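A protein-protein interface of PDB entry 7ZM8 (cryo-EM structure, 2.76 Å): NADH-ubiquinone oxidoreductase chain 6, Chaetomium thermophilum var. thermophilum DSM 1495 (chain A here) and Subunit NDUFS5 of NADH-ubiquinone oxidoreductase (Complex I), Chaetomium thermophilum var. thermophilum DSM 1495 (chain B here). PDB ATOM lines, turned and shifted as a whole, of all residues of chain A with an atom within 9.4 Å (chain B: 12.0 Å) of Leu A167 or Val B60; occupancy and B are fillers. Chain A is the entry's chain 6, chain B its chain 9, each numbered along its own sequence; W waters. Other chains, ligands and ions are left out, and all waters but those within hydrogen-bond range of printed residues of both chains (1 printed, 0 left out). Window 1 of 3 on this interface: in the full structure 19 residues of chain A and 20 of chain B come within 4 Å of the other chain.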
ATOM      1  N   LEU A   7     -35.489   4.200  30.039  1.00  0.00           N
ATOM      2  CA  LEU A   7     -35.071   4.020  28.630  1.00  0.00           C
ATOM      3  C   LEU A   7     -36.167   3.244  27.909  1.00  0.00           C
ATOM      4  O   LEU A   7     -36.542   2.182  28.402  1.00  0.00           O
ATOM      5  CB  LEU A   7     -33.731   3.282  28.568  1.00  0.00           C
ATOM      6  CG  LEU A   7     -32.539   3.977  29.215  1.00  0.00           C
ATOM      7  CD1 LEU A   7     -31.336   3.049  29.210  1.00  0.00           C
ATOM      8  CD2 LEU A   7     -32.214   5.277  28.498  1.00  0.00           C
ATOM      9  N   TYR A 127     -11.019   0.202  15.197  1.00  0.00           N
ATOM     10  CA  TYR A 127     -12.197  -0.421  15.855  1.00  0.00           C
ATOM     11  C   TYR A 127     -13.475  -0.259  15.024  1.00  0.00           C
ATOM     12  O   TYR A 127     -14.251  -1.222  14.947  1.00  0.00           O
ATOM     13  CB  TYR A 127     -12.404   0.117  17.267  1.00  0.00           C
ATOM     14  CG  TYR A 127     -13.021  -0.905  18.184  1.00  0.00           C
ATOM     15  CD1 TYR A 127     -12.403  -2.127  18.380  1.00  0.00           C
ATOM     16  CD2 TYR A 127     -14.224  -0.671  18.830  1.00  0.00           C
ATOM     17  CE1 TYR A 127     -12.954  -3.090  19.206  1.00  0.00           C
ATOM     18  CE2 TYR A 127     -14.787  -1.623  19.662  1.00  0.00           C
ATOM     19  CZ  TYR A 127     -14.150  -2.837  19.849  1.00  0.00           C
ATOM     20  OH  TYR A 127     -14.687  -3.794  20.659  1.00  0.00           O
ATOM     21  N   ILE A 130     -14.217  -2.914  12.336  1.00  0.00           N
ATOM     22  CA  ILE A 130     -14.558  -4.231  12.858  1.00  0.00           C
ATOM     23  C   ILE A 130     -15.586  -4.143  13.988  1.00  0.00           C
ATOM     24  O   ILE A 130     -15.725  -5.083  14.769  1.00  0.00           O
ATOM     25  CB  ILE A 130     -13.305  -4.997  13.308  1.00  0.00           C
ATOM     26  CG1 ILE A 130     -12.609  -4.257  14.452  1.00  0.00           C
ATOM     27  CG2 ILE A 130     -12.354  -5.191  12.141  1.00  0.00           C
ATOM     28  CD1 ILE A 130     -11.468  -5.032  15.071  1.00  0.00           C
ATOM     29  N   ILE A 131     -16.314  -3.027  14.087  1.00  0.00           N
ATOM     30  CA  ILE A 131     -17.331  -2.890  15.124  1.00  0.00           C
ATOM     31  C   ILE A 131     -18.454  -3.905  14.951  1.00  0.00           C
ATOM     32  O   ILE A 131     -19.104  -4.278  15.933  1.00  0.00           O
ATOM     33  CB  ILE A 131     -17.882  -1.450  15.142  1.00  0.00           C
ATOM     34  CG1 ILE A 131     -18.714  -1.197  16.404  1.00  0.00           C
ATOM     35  CG2 ILE A 131     -18.700  -1.166  13.890  1.00  0.00           C
ATOM     36  CD1 ILE A 131     -17.967  -1.411  17.694  1.00  0.00           C
ATOM     37  N   SER A 132     -18.694  -4.375  13.730  1.00  0.00           N
ATOM     38  CA  SER A 132     -19.755  -5.343  13.475  1.00  0.00           C
ATOM     39  C   SER A 132     -19.183  -6.665  12.974  1.00  0.00           C
ATOM     40  O   SER A 132     -19.438  -7.073  11.840  1.00  0.00           O
ATOM     41  CB  SER A 132     -20.757  -4.783  12.465  1.00  0.00           C
ATOM     42  OG  SER A 132     -20.127  -4.480  11.232  1.00  0.00           O
ATOM     43  N   LYS A 164     -27.308 -12.193  24.040  1.00  0.00           N
ATOM     44  CA  LYS A 164     -26.036 -11.490  23.932  1.00  0.00           C
ATOM     45  C   LYS A 164     -26.261  -9.995  23.738  1.00  0.00           C
ATOM     46  O   LYS A 164     -26.864  -9.578  22.749  1.00  0.00           O
ATOM     47  CB  LYS A 164     -25.207 -12.047  22.773  1.00  0.00           C
ATOM     48  CG  LYS A 164     -26.027 -12.442  21.553  1.00  0.00           C
ATOM     49  CD  LYS A 164     -25.146 -13.002  20.448  1.00  0.00           C
ATOM     50  CE  LYS A 164     -25.969 -13.399  19.232  1.00  0.00           C
ATOM     51  NZ  LYS A 164     -25.117 -13.950  18.140  1.00  0.00           N
ATOM     52  N   ASN A 165     -25.781  -9.190  24.683  1.00  0.00           N
ATOM     53  CA  ASN A 165     -25.903  -7.745  24.546  1.00  0.00           C
ATOM     54  C   ASN A 165     -25.042  -7.263  23.387  1.00  0.00           C
ATOM     55  O   ASN A 165     -23.937  -7.764  23.167  1.00  0.00           O
ATOM     56  CB  ASN A 165     -25.494  -7.038  25.840  1.00  0.00           C
ATOM     57  CG  ASN A 165     -24.035  -7.252  26.187  1.00  0.00           C
ATOM     58  OD1 ASN A 165     -23.468  -8.312  25.916  1.00  0.00           O
ATOM     59  ND2 ASN A 165     -23.416  -6.239  26.785  1.00  0.00           N
ATOM     60  N   ASP A 166     -25.559  -6.296  22.639  1.00  0.00           N
ATOM     61  CA  ASP A 166     -24.855  -5.744  21.494  1.00  0.00           C
ATOM     62  C   ASP A 166     -24.896  -4.228  21.556  1.00  0.00           C
ATOM     63  O   ASP A 166     -25.882  -3.641  22.008  1.00  0.00           O
ATOM     64  CB  ASP A 166     -25.466  -6.232  20.175  1.00  0.00           C
ATOM     65  CG  ASP A 166     -24.424  -6.449  19.099  1.00  0.00           C
ATOM     66  OD1 ASP A 166     -23.392  -5.749  19.121  1.00  0.00           O
ATOM     67  OD2 ASP A 166     -24.638  -7.320  18.230  1.00  0.00           O
ATOM     68  N   LEU A 167     -23.814  -3.602  21.110  1.00  0.00           N
ATOM     69  CA  LEU A 167     -23.762  -2.155  21.034  1.00  0.00           C
ATOM     70  C   LEU A 167     -24.698  -1.644  19.954  1.00  0.00           C
ATOM     71  O   LEU A 167     -24.901  -2.284  18.923  1.00  0.00           O
ATOM     72  CB  LEU A 167     -22.346  -1.689  20.730  1.00  0.00           C
ATOM     73  CG  LEU A 167     -21.353  -1.634  21.877  1.00  0.00           C
ATOM     74  CD1 LEU A 167     -19.989  -1.345  21.319  1.00  0.00           C
ATOM     75  CD2 LEU A 167     -21.767  -0.572  22.859  1.00  0.00           C
ATOM     76  N   PHE A 168     -25.282  -0.478  20.210  1.00  0.00           N
ATOM     77  CA  PHE A 168     -26.087   0.172  19.153  1.00  0.00           C
ATOM     78  C   PHE A 168     -25.467   1.553  18.960  1.00  0.00           C
ATOM     79  O   PHE A 168     -24.971   2.104  19.938  1.00  0.00           O
ATOM     80  CB  PHE A 168     -27.557   0.262  19.567  1.00  0.00           C
ATOM     81  CG  PHE A 168     -28.392  -0.956  19.268  1.00  0.00           C
ATOM     82  CD1 PHE A 168     -28.412  -2.037  20.133  1.00  0.00           C
ATOM     83  CD2 PHE A 168     -29.178  -1.013  18.129  1.00  0.00           C
ATOM     84  CE1 PHE A 168     -29.186  -3.152  19.860  1.00  0.00           C
ATOM     85  CE2 PHE A 168     -29.952  -2.129  17.856  1.00  0.00           C
ATOM     86  CZ  PHE A 168     -29.955  -3.196  18.722  1.00  0.00           C
ATOM     87  N   PHE A 169     -25.529   2.095  17.746  1.00  0.00           N
ATOM     88  CA  PHE A 169     -24.957   3.433  17.454  1.00  0.00           C
ATOM     89  C   PHE A 169     -26.061   4.475  17.604  1.00  0.00           C
ATOM     90  O   PHE A 169     -27.027   4.432  16.842  1.00  0.00           O
ATOM     91  CB  PHE A 169     -24.393   3.469  16.034  1.00  0.00           C
ATOM     92  CG  PHE A 169     -23.049   2.817  15.866  1.00  0.00           C
ATOM     93  CD1 PHE A 169     -21.885   3.535  16.083  1.00  0.00           C
ATOM     94  CD2 PHE A 169     -22.948   1.490  15.484  1.00  0.00           C
ATOM     95  CE1 PHE A 169     -20.647   2.937  15.924  1.00  0.00           C
ATOM     96  CE2 PHE A 169     -21.710   0.894  15.327  1.00  0.00           C
ATOM     97  CZ  PHE A 169     -20.563   1.619  15.546  1.00  0.00           C
ATOM     98  N   ILE A 170     -25.909   5.379  18.566  1.00  0.00           N
ATOM     99  CA  ILE A 170     -26.940   6.427  18.824  1.00  0.00           C
ATOM    100  C   ILE A 170     -26.631   7.683  18.005  1.00  0.00           C
ATOM    101  O   ILE A 170     -25.451   8.006  17.844  1.00  0.00           O
ATOM    102  CB  ILE A 170     -27.110   6.710  20.334  1.00  0.00           C
ATOM    103  CG1 ILE A 170     -28.398   7.477  20.642  1.00  0.00           C
ATOM    104  CG2 ILE A 170     -25.887   7.383  20.934  1.00  0.00           C
ATOM    105  CD1 ILE A 170     -29.608   6.594  20.792  1.00  0.00           C
ATOM    106  N   GLU B  49      -9.262   8.037  20.872  1.00  0.00           N
ATOM    107  CA  GLU B  49     -10.573   7.569  21.358  1.00  0.00           C
ATOM    108  C   GLU B  49     -11.672   8.258  20.566  1.00  0.00           C
ATOM    109  O   GLU B  49     -12.693   7.637  20.308  1.00  0.00           O
ATOM    110  CB  GLU B  49     -10.697   7.914  22.839  1.00  0.00           C
ATOM    111  CG  GLU B  49     -12.073   7.703  23.429  1.00  0.00           C
ATOM    112  CD  GLU B  49     -12.547   6.264  23.451  1.00  0.00           C
ATOM    113  OE1 GLU B  49     -11.719   5.366  23.263  1.00  0.00           O
ATOM    114  OE2 GLU B  49     -13.746   6.050  23.656  1.00  0.00           O
ATOM    115  N   HIS B  52     -11.721   6.169  17.220  1.00  0.00           N
ATOM    116  CA  HIS B  52     -12.075   4.727  17.290  1.00  0.00           C
ATOM    117  C   HIS B  52     -13.114   4.334  18.338  1.00  0.00           C
ATOM    118  O   HIS B  52     -13.669   3.260  18.149  1.00  0.00           O
ATOM    119  CB  HIS B  52     -10.804   3.894  17.366  1.00  0.00           C
ATOM    120  CG  HIS B  52      -9.753   4.280  16.384  1.00  0.00           C
ATOM    121  ND1 HIS B  52      -9.932   4.156  15.028  1.00  0.00           N
ATOM    122  CD2 HIS B  52      -8.508   4.763  16.561  1.00  0.00           C
ATOM    123  CE1 HIS B  52      -8.849   4.565  14.407  1.00  0.00           C
ATOM    124  NE2 HIS B  52      -7.962   4.937  15.324  1.00  0.00           N
ATOM    125  N   HIS B  53     -13.339   5.116  19.396  1.00  0.00           N
ATOM    126  CA  HIS B  53     -14.427   4.855  20.391  1.00  0.00           C
ATOM    127  C   HIS B  53     -14.352   3.486  21.046  1.00  0.00           C
ATOM    128  O   HIS B  53     -15.400   2.959  21.353  1.00  0.00           O
ATOM    129  CB  HIS B  53     -15.830   4.999  19.799  1.00  0.00           C
ATOM    130  CG  HIS B  53     -16.019   6.212  18.959  1.00  0.00           C
ATOM    131  ND1 HIS B  53     -16.068   6.145  17.589  1.00  0.00           N
ATOM    132  CD2 HIS B  53     -16.171   7.506  19.290  1.00  0.00           C
ATOM    133  CE1 HIS B  53     -16.230   7.351  17.108  1.00  0.00           C
ATOM    134  NE2 HIS B  53     -16.299   8.202  18.130  1.00  0.00           N
ATOM    135  N   ARG B  54     -13.158   2.930  21.199  1.00  0.00           N
ATOM    136  CA  ARG B  54     -12.960   1.633  21.883  1.00  0.00           C
ATOM    137  C   ARG B  54     -13.299   1.706  23.380  1.00  0.00           C
ATOM    138  O   ARG B  54     -14.086   0.881  23.816  1.00  0.00           O
ATOM    139  CB  ARG B  54     -11.545   1.151  21.550  1.00  0.00           C
ATOM    140  CG  ARG B  54     -11.116  -0.140  22.223  1.00  0.00           C
ATOM    141  CD  ARG B  54      -9.687  -0.478  21.845  1.00  0.00           C
ATOM    142  NE  ARG B  54      -9.226  -1.663  22.551  1.00  0.00           N
ATOM    143  CZ  ARG B  54      -9.344  -2.905  22.095  1.00  0.00           C
ATOM    144  NH1 ARG B  54      -8.893  -3.919  22.814  1.00  0.00           N
ATOM    145  NH2 ARG B  54      -9.908  -3.130  20.923  1.00  0.00           N
ATOM    146  N   LYS B  55     -12.801   2.692  24.124  1.00  0.00           N
ATOM    147  CA  LYS B  55     -13.038   2.773  25.589  1.00  0.00           C
ATOM    148  C   LYS B  55     -14.522   3.019  25.870  1.00  0.00           C
ATOM    149  O   LYS B  55     -15.013   2.484  26.858  1.00  0.00           O
ATOM    150  CB  LYS B  55     -12.146   3.832  26.242  1.00  0.00           C
ATOM    151  CG  LYS B  55     -10.680   3.808  25.860  1.00  0.00           C
ATOM    152  CD  LYS B  55      -9.955   5.041  26.325  1.00  0.00           C
ATOM    153  CE  LYS B  55     -10.262   5.384  27.764  1.00  0.00           C
ATOM    154  NZ  LYS B  55      -9.665   4.415  28.710  1.00  0.00           N
ATOM    155  N   GLU B  56     -15.188   3.859  25.067  1.00  0.00           N
ATOM    156  CA  GLU B  56     -16.638   4.131  25.213  1.00  0.00           C
ATOM    157  C   GLU B  56     -17.446   2.871  24.949  1.00  0.00           C
ATOM    158  O   GLU B  56     -18.423   2.641  25.662  1.00  0.00           O
ATOM    159  CB  GLU B  56     -17.046   5.163  24.181  1.00  0.00           C
ATOM    160  CG  GLU B  56     -18.475   5.633  24.354  1.00  0.00           C
ATOM    161  CD  GLU B  56     -18.978   6.560  23.266  1.00  0.00           C
ATOM    162  OE1 GLU B  56     -20.197   6.620  23.076  1.00  0.00           O
ATOM    163  OE2 GLU B  56     -18.152   7.217  22.622  1.00  0.00           O
ATOM    164  N   ALA B  57     -17.073   2.115  23.926  1.00  0.00           N
ATOM    165  CA  ALA B  57     -17.744   0.845  23.602  1.00  0.00           C
ATOM    166  C   ALA B  57     -17.625  -0.084  24.799  1.00  0.00           C
ATOM    167  O   ALA B  57     -18.600  -0.753  25.124  1.00  0.00           O
ATOM    168  CB  ALA B  57     -17.058   0.286  22.397  1.00  0.00           C
ATOM    169  N   ALA B  58     -16.450  -0.119  25.408  1.00  0.00           N
ATOM    170  CA  ALA B  58     -16.197  -0.972  26.585  1.00  0.00           C
ATOM    171  C   ALA B  58     -17.054  -0.543  27.774  1.00  0.00           C
ATOM    172  O   ALA B  58     -17.605  -1.435  28.441  1.00  0.00           O
ATOM    173  CB  ALA B  58     -14.744  -0.905  26.922  1.00  0.00           C
ATOM    174  N   ARG B  59     -17.178   0.759  28.015  1.00  0.00           N
ATOM    175  CA  ARG B  59     -18.059   1.234  29.106  1.00  0.00           C
ATOM    176  C   ARG B  59     -19.493   0.814  28.816  1.00  0.00           C
ATOM    177  O   ARG B  59     -20.139   0.320  29.734  1.00  0.00           O
ATOM    178  CB  ARG B  59     -18.021   2.760  29.203  1.00  0.00           C
ATOM    179  CG  ARG B  59     -19.022   3.354  30.182  1.00  0.00           C
ATOM    180  CD  ARG B  59     -18.961   4.866  30.218  1.00  0.00           C
ATOM    181  NE  ARG B  59     -20.061   5.448  30.969  1.00  0.00           N
ATOM    182  CZ  ARG B  59     -21.195   5.872  30.428  1.00  0.00           C
ATOM    183  NH1 ARG B  59     -21.374   5.786  29.121  1.00  0.00           N
ATOM    184  NH2 ARG B  59     -22.141   6.389  31.193  1.00  0.00           N
ATOM    185  N   VAL B  60     -19.961   1.003  27.587  1.00  0.00           N
ATOM    186  CA  VAL B  60     -21.383   0.703  27.256  1.00  0.00           C
ATOM    187  C   VAL B  60     -21.647  -0.799  27.322  1.00  0.00           C
ATOM    188  O   VAL B  60     -22.695  -1.171  27.811  1.00  0.00           O
ATOM    189  CB  VAL B  60     -21.889   1.392  25.969  1.00  0.00           C
ATOM    190  CG1 VAL B  60     -23.348   1.072  25.693  1.00  0.00           C
ATOM    191  CG2 VAL B  60     -21.698   2.899  26.018  1.00  0.00           C
ATOM    192  N   ARG B  61     -20.725  -1.630  26.873  1.00  0.00           N
ATOM    193  CA  ARG B  61     -21.025  -3.078  26.845  1.00  0.00           C
ATOM    194  C   ARG B  61     -21.256  -3.522  28.281  1.00  0.00           C
ATOM    195  O   ARG B  61     -22.170  -4.325  28.503  1.00  0.00           O
ATOM    196  CB  ARG B  61     -19.932  -3.839  26.087  1.00  0.00           C
ATOM    197  CG  ARG B  61     -20.175  -3.921  24.587  1.00  0.00           C
ATOM    198  CD  ARG B  61     -19.169  -4.759  23.821  1.00  0.00           C
ATOM    199  NE  ARG B  61     -18.179  -3.962  23.112  1.00  0.00           N
ATOM    200  CZ  ARG B  61     -16.963  -3.685  23.568  1.00  0.00           C
ATOM    201  NH1 ARG B  61     -16.566  -4.150  24.740  1.00  0.00           N
ATOM    202  NH2 ARG B  61     -16.142  -2.949  22.845  1.00  0.00           N
ATOM    203  N   ALA B  62     -20.462  -3.005  29.214  1.00  0.00           N
ATOM    204  CA  ALA B  62     -20.581  -3.328  30.650  1.00  0.00           C
ATOM    205  C   ALA B  62     -21.858  -2.736  31.231  1.00  0.00           C
ATOM    206  O   ALA B  62     -22.589  -3.454  31.898  1.00  0.00           O
ATOM    207  CB  ALA B  62     -19.413  -2.687  31.318  1.00  0.00           C
ATOM    208  N   LEU B  63     -22.049  -1.442  31.045  1.00  0.00           N
ATOM    209  CA  LEU B  63     -23.217  -0.777  31.607  1.00  0.00           C
ATOM    210  C   LEU B  63     -24.503  -1.352  31.031  1.00  0.00           C
ATOM    211  O   LEU B  63     -25.520  -1.437  31.727  1.00  0.00           O
ATOM    212  CB  LEU B  63     -23.129   0.724  31.344  1.00  0.00           C
ATOM    213  CG  LEU B  63     -24.259   1.610  31.865  1.00  0.00           C
ATOM    214  CD1 LEU B  63     -24.624   1.245  33.294  1.00  0.00           C
ATOM    215  CD2 LEU B  63     -23.875   3.073  31.763  1.00  0.00           C
ATOM    216  N   GLN B  64     -24.476  -1.741  29.760  1.00  0.00           N
ATOM    217  CA  GLN B  64     -25.640  -2.344  29.131  1.00  0.00           C
ATOM    218  C   GLN B  64     -25.907  -3.737  29.675  1.00  0.00           C
ATOM    219  O   GLN B  64     -27.064  -4.152  29.772  1.00  0.00           O
ATOM    220  CB  GLN B  64     -25.414  -2.390  27.626  1.00  0.00           C
ATOM    221  CG  GLN B  64     -26.534  -2.895  26.776  1.00  0.00           C
ATOM    222  CD  GLN B  64     -26.143  -2.813  25.331  1.00  0.00           C
ATOM    223  OE1 GLN B  64     -26.938  -3.143  24.458  1.00  0.00           O
ATOM    224  NE2 GLN B  64     -24.928  -2.398  25.061  1.00  0.00           N
ATOM    225  N   ALA B  65     -24.852  -4.472  30.028  1.00  0.00           N
ATOM    226  CA  ALA B  65     -25.029  -5.802  30.595  1.00  0.00           C
ATOM    227  C   ALA B  65     -25.563  -5.730  32.017  1.00  0.00           C
ATOM    228  O   ALA B  65     -26.314  -6.610  32.450  1.00  0.00           O
ATOM    229  CB  ALA B  65     -23.710  -6.566  30.551  1.00  0.00           C
ATOM    230  N   ALA B  66     -25.177  -4.698  32.765  1.00  0.00           N
ATOM    231  CA  ALA B  66     -25.742  -4.506  34.092  1.00  0.00           C
ATOM    232  C   ALA B  66     -27.176  -4.011  34.017  1.00  0.00           C
ATOM    233  O   ALA B  66     -27.999  -4.365  34.867  1.00  0.00           O
ATOM    234  CB  ALA B  66     -24.890  -3.528  34.892  1.00  0.00           C
ATOM    235  N   TYR B  67     -27.485  -3.183  33.023  1.00  0.00           N
ATOM    236  CA  TYR B  67     -28.834  -2.650  32.885  1.00  0.00           C
ATOM    237  C   TYR B  67     -29.815  -3.747  32.506  1.00  0.00           C
ATOM    238  O   TYR B  67     -30.913  -3.834  33.064  1.00  0.00           O
ATOM    239  CB  TYR B  67     -28.835  -1.532  31.845  1.00  0.00           C
ATOM    240  CG  TYR B  67     -30.197  -0.981  31.512  1.00  0.00           C
ATOM    241  CD1 TYR B  67     -30.848  -0.122  32.378  1.00  0.00           C
ATOM    242  CD2 TYR B  67     -30.825  -1.305  30.322  1.00  0.00           C
ATOM    243  CE1 TYR B  67     -32.082   0.383  32.077  1.00  0.00           C
ATOM    244  CE2 TYR B  67     -32.060  -0.804  30.014  1.00  0.00           C
ATOM    245  CZ  TYR B  67     -32.684   0.038  30.895  1.00  0.00           C
ATOM    246  OH  TYR B  67     -33.924   0.546  30.586  1.00  0.00           O
ATOM    247  N   ARG B  68     -29.435  -4.594  31.555  1.00  0.00           N
ATOM    248  CA  ARG B  68     -30.324  -5.663  31.131  1.00  0.00           C
ATOM    249  C   ARG B  68     -30.499  -6.720  32.211  1.00  0.00           C
ATOM    250  O   ARG B  68     -31.601  -7.249  32.376  1.00  0.00           O
ATOM    251  CB  ARG B  68     -29.815  -6.275  29.829  1.00  0.00           C
ATOM    252  CG  ARG B  68     -30.435  -5.641  28.600  1.00  0.00           C
ATOM    253  CD  ARG B  68     -29.738  -6.045  27.323  1.00  0.00           C
ATOM    254  NE  ARG B  68     -29.734  -4.964  26.349  1.00  0.00           N
ATOM    255  CZ  ARG B  68     -29.553  -5.144  25.048  1.00  0.00           C
ATOM    256  NH1 ARG B  68     -29.594  -4.116  24.219  1.00  0.00           N
ATOM    257  NH2 ARG B  68     -29.335  -6.358  24.572  1.00  0.00           N
ATOM    258  N   GLU B  69     -29.447  -7.032  32.960  1.00  0.00           N
ATOM    259  CA  GLU B  69     -29.569  -7.986  34.053  1.00  0.00           C
ATOM    260  C   GLU B  69     -30.303  -7.412  35.254  1.00  0.00           C
ATOM    261  O   GLU B  69     -30.666  -8.172  36.155  1.00  0.00           O
ATOM    262  CB  GLU B  69     -28.187  -8.479  34.485  1.00  0.00           C
ATOM    263  CG  GLU B  69     -27.455  -7.528  35.404  1.00  0.00           C
ATOM    264  CD  GLU B  69     -26.249  -8.167  36.060  1.00  0.00           C
ATOM    265  OE1 GLU B  69     -26.195  -9.412  36.121  1.00  0.00           O
ATOM    266  OE2 GLU B  69     -25.353  -7.422  36.509  1.00  0.00           O
ATOM    267  N   ALA B  70     -30.530  -6.101  35.288  1.00  0.00           N
ATOM    268  CA  ALA B  70     -31.289  -5.462  36.352  1.00  0.00           C
ATOM    269  C   ALA B  70     -32.762  -5.301  36.014  1.00  0.00           C
ATOM    270  O   ALA B  70     -33.610  -5.430  36.899  1.00  0.00           O
ATOM    271  CB  ALA B  70     -30.692  -4.092  36.682  1.00  0.00           C
ATOM    272  N   GLU B  71     -33.088  -5.017  34.756  1.00  0.00           N
ATOM    273  CA  GLU B  71     -34.474  -4.897  34.323  1.00  0.00           C
ATOM    274  C   GLU B  71     -35.063  -6.206  33.822  1.00  0.00           C
ATOM    275  O   GLU B  71     -36.211  -6.216  33.368  1.00  0.00           O
ATOM    276  CB  GLU B  71     -34.603  -3.826  33.235  1.00  0.00           C
ATOM    277  CG  GLU B  71     -34.987  -2.445  33.751  1.00  0.00           C
ATOM    278  CD  GLU B  71     -33.810  -1.665  34.300  1.00  0.00           C
ATOM    279  OE1 GLU B  71     -32.686  -2.203  34.300  1.00  0.00           O
ATOM    280  OE2 GLU B  71     -34.010  -0.509  34.727  1.00  0.00           O
HETATM  281  O   HOH W   1     -26.944  -0.848  22.802  1.00  0.00           O
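Among the printed residues, merely in contact across the chains: Leu A7 with Tyr B67 (3.4 Å), Tyr A127 with Arg B54 (3.5 Å), Tyr A127 with His B52 (3.5 Å), Leu A167 with Ala B57 (3.5 Å), Leu A167 with Val B60 (3.6 Å), Leu A167 with Arg B61 (3.7 Å), Asn A165 with Arg B68 (3.7 Å) and Asn A165 with Ala B65 (3.8 Å).
OH of Tyr A127 is in hydrogen-bond range of NH2 of Arg B61. The side-chain amide nitrogen (ND2) of Asn A165 is in hydrogen-bond range of the backbone carbonyl oxygen (O) of Arg B61 (2.9 Å). The side-chain amide oxygen (OE1) of Gln B64 sits close to the backbone carbonyl oxygen (O) of Asp A166, 2.7 Å away.
Water W1 lies within hydrogen-bond range of OE1 of Gln B64 (2.8 Å), O of Asp A166 (3.1 Å) and N of Phe A168 (3.1 Å).
Printed residues of chain B that touch a printed residue of chain A: His B52, Arg B54, Ala B57, Val B60, Arg B61, Gln B64, Ala B65, Tyr B67 and Arg B68. Hydrophobic or aromatic side chains of chain B within 4 Å of the printed part of chain A: Ala B57, Val B60, Ala B65 and Tyr B67. Of the 12 printed residues of chain A, 5 touch a printed residue of chain B. Hydrophobic or aromatic side chains of chain A that line the printed part of chain B: Leu A7, Tyr A127 and Leu A167. Along chain A the printed residues that touch a printed residue of chain B span positions 7 to 167.
Of chain B, only Ala B57, Val B60 and Arg B61 come within 4 Å of Leu A167. Of chain A, only Leu A167 (3.6 Å) comes within 4 Å of Val B60. Asn A165 touches just these residues of chain B: Arg B61, Ala B65 and Arg B68. Asp A166 touches one residue of chain B. No residue of chain B comes within 4 Å of Phe A168. Of the printed residues of chain B, Tyr A127 touches His B52 (3.5 Å), Arg B54 (3.5 Å) and Arg B61 (2.8 Å). Of the printed residues of chain A, Arg B54 touches Tyr A127 (3.5 Å). Printed residues of chain A within 4 Å of Ala B65: Asn A165. Of the printed residues of chain A, Arg B68 touches Asn A165. Leu B63 touches none of the printed residues of chain A. The nearest residue of chain B that does not touch Leu A167 is Gln B64 (4.2 Å). The nearest residue of chain A that does not touch Val B60 is Asn A165 (5.2 Å).
OE1 of Gln B64 is in hydrogen-bond range of NH1 of Arg B68 (2.8 Å). O of Tyr B67 lies close to OE1 of Glu B71, 2.7 Å away.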
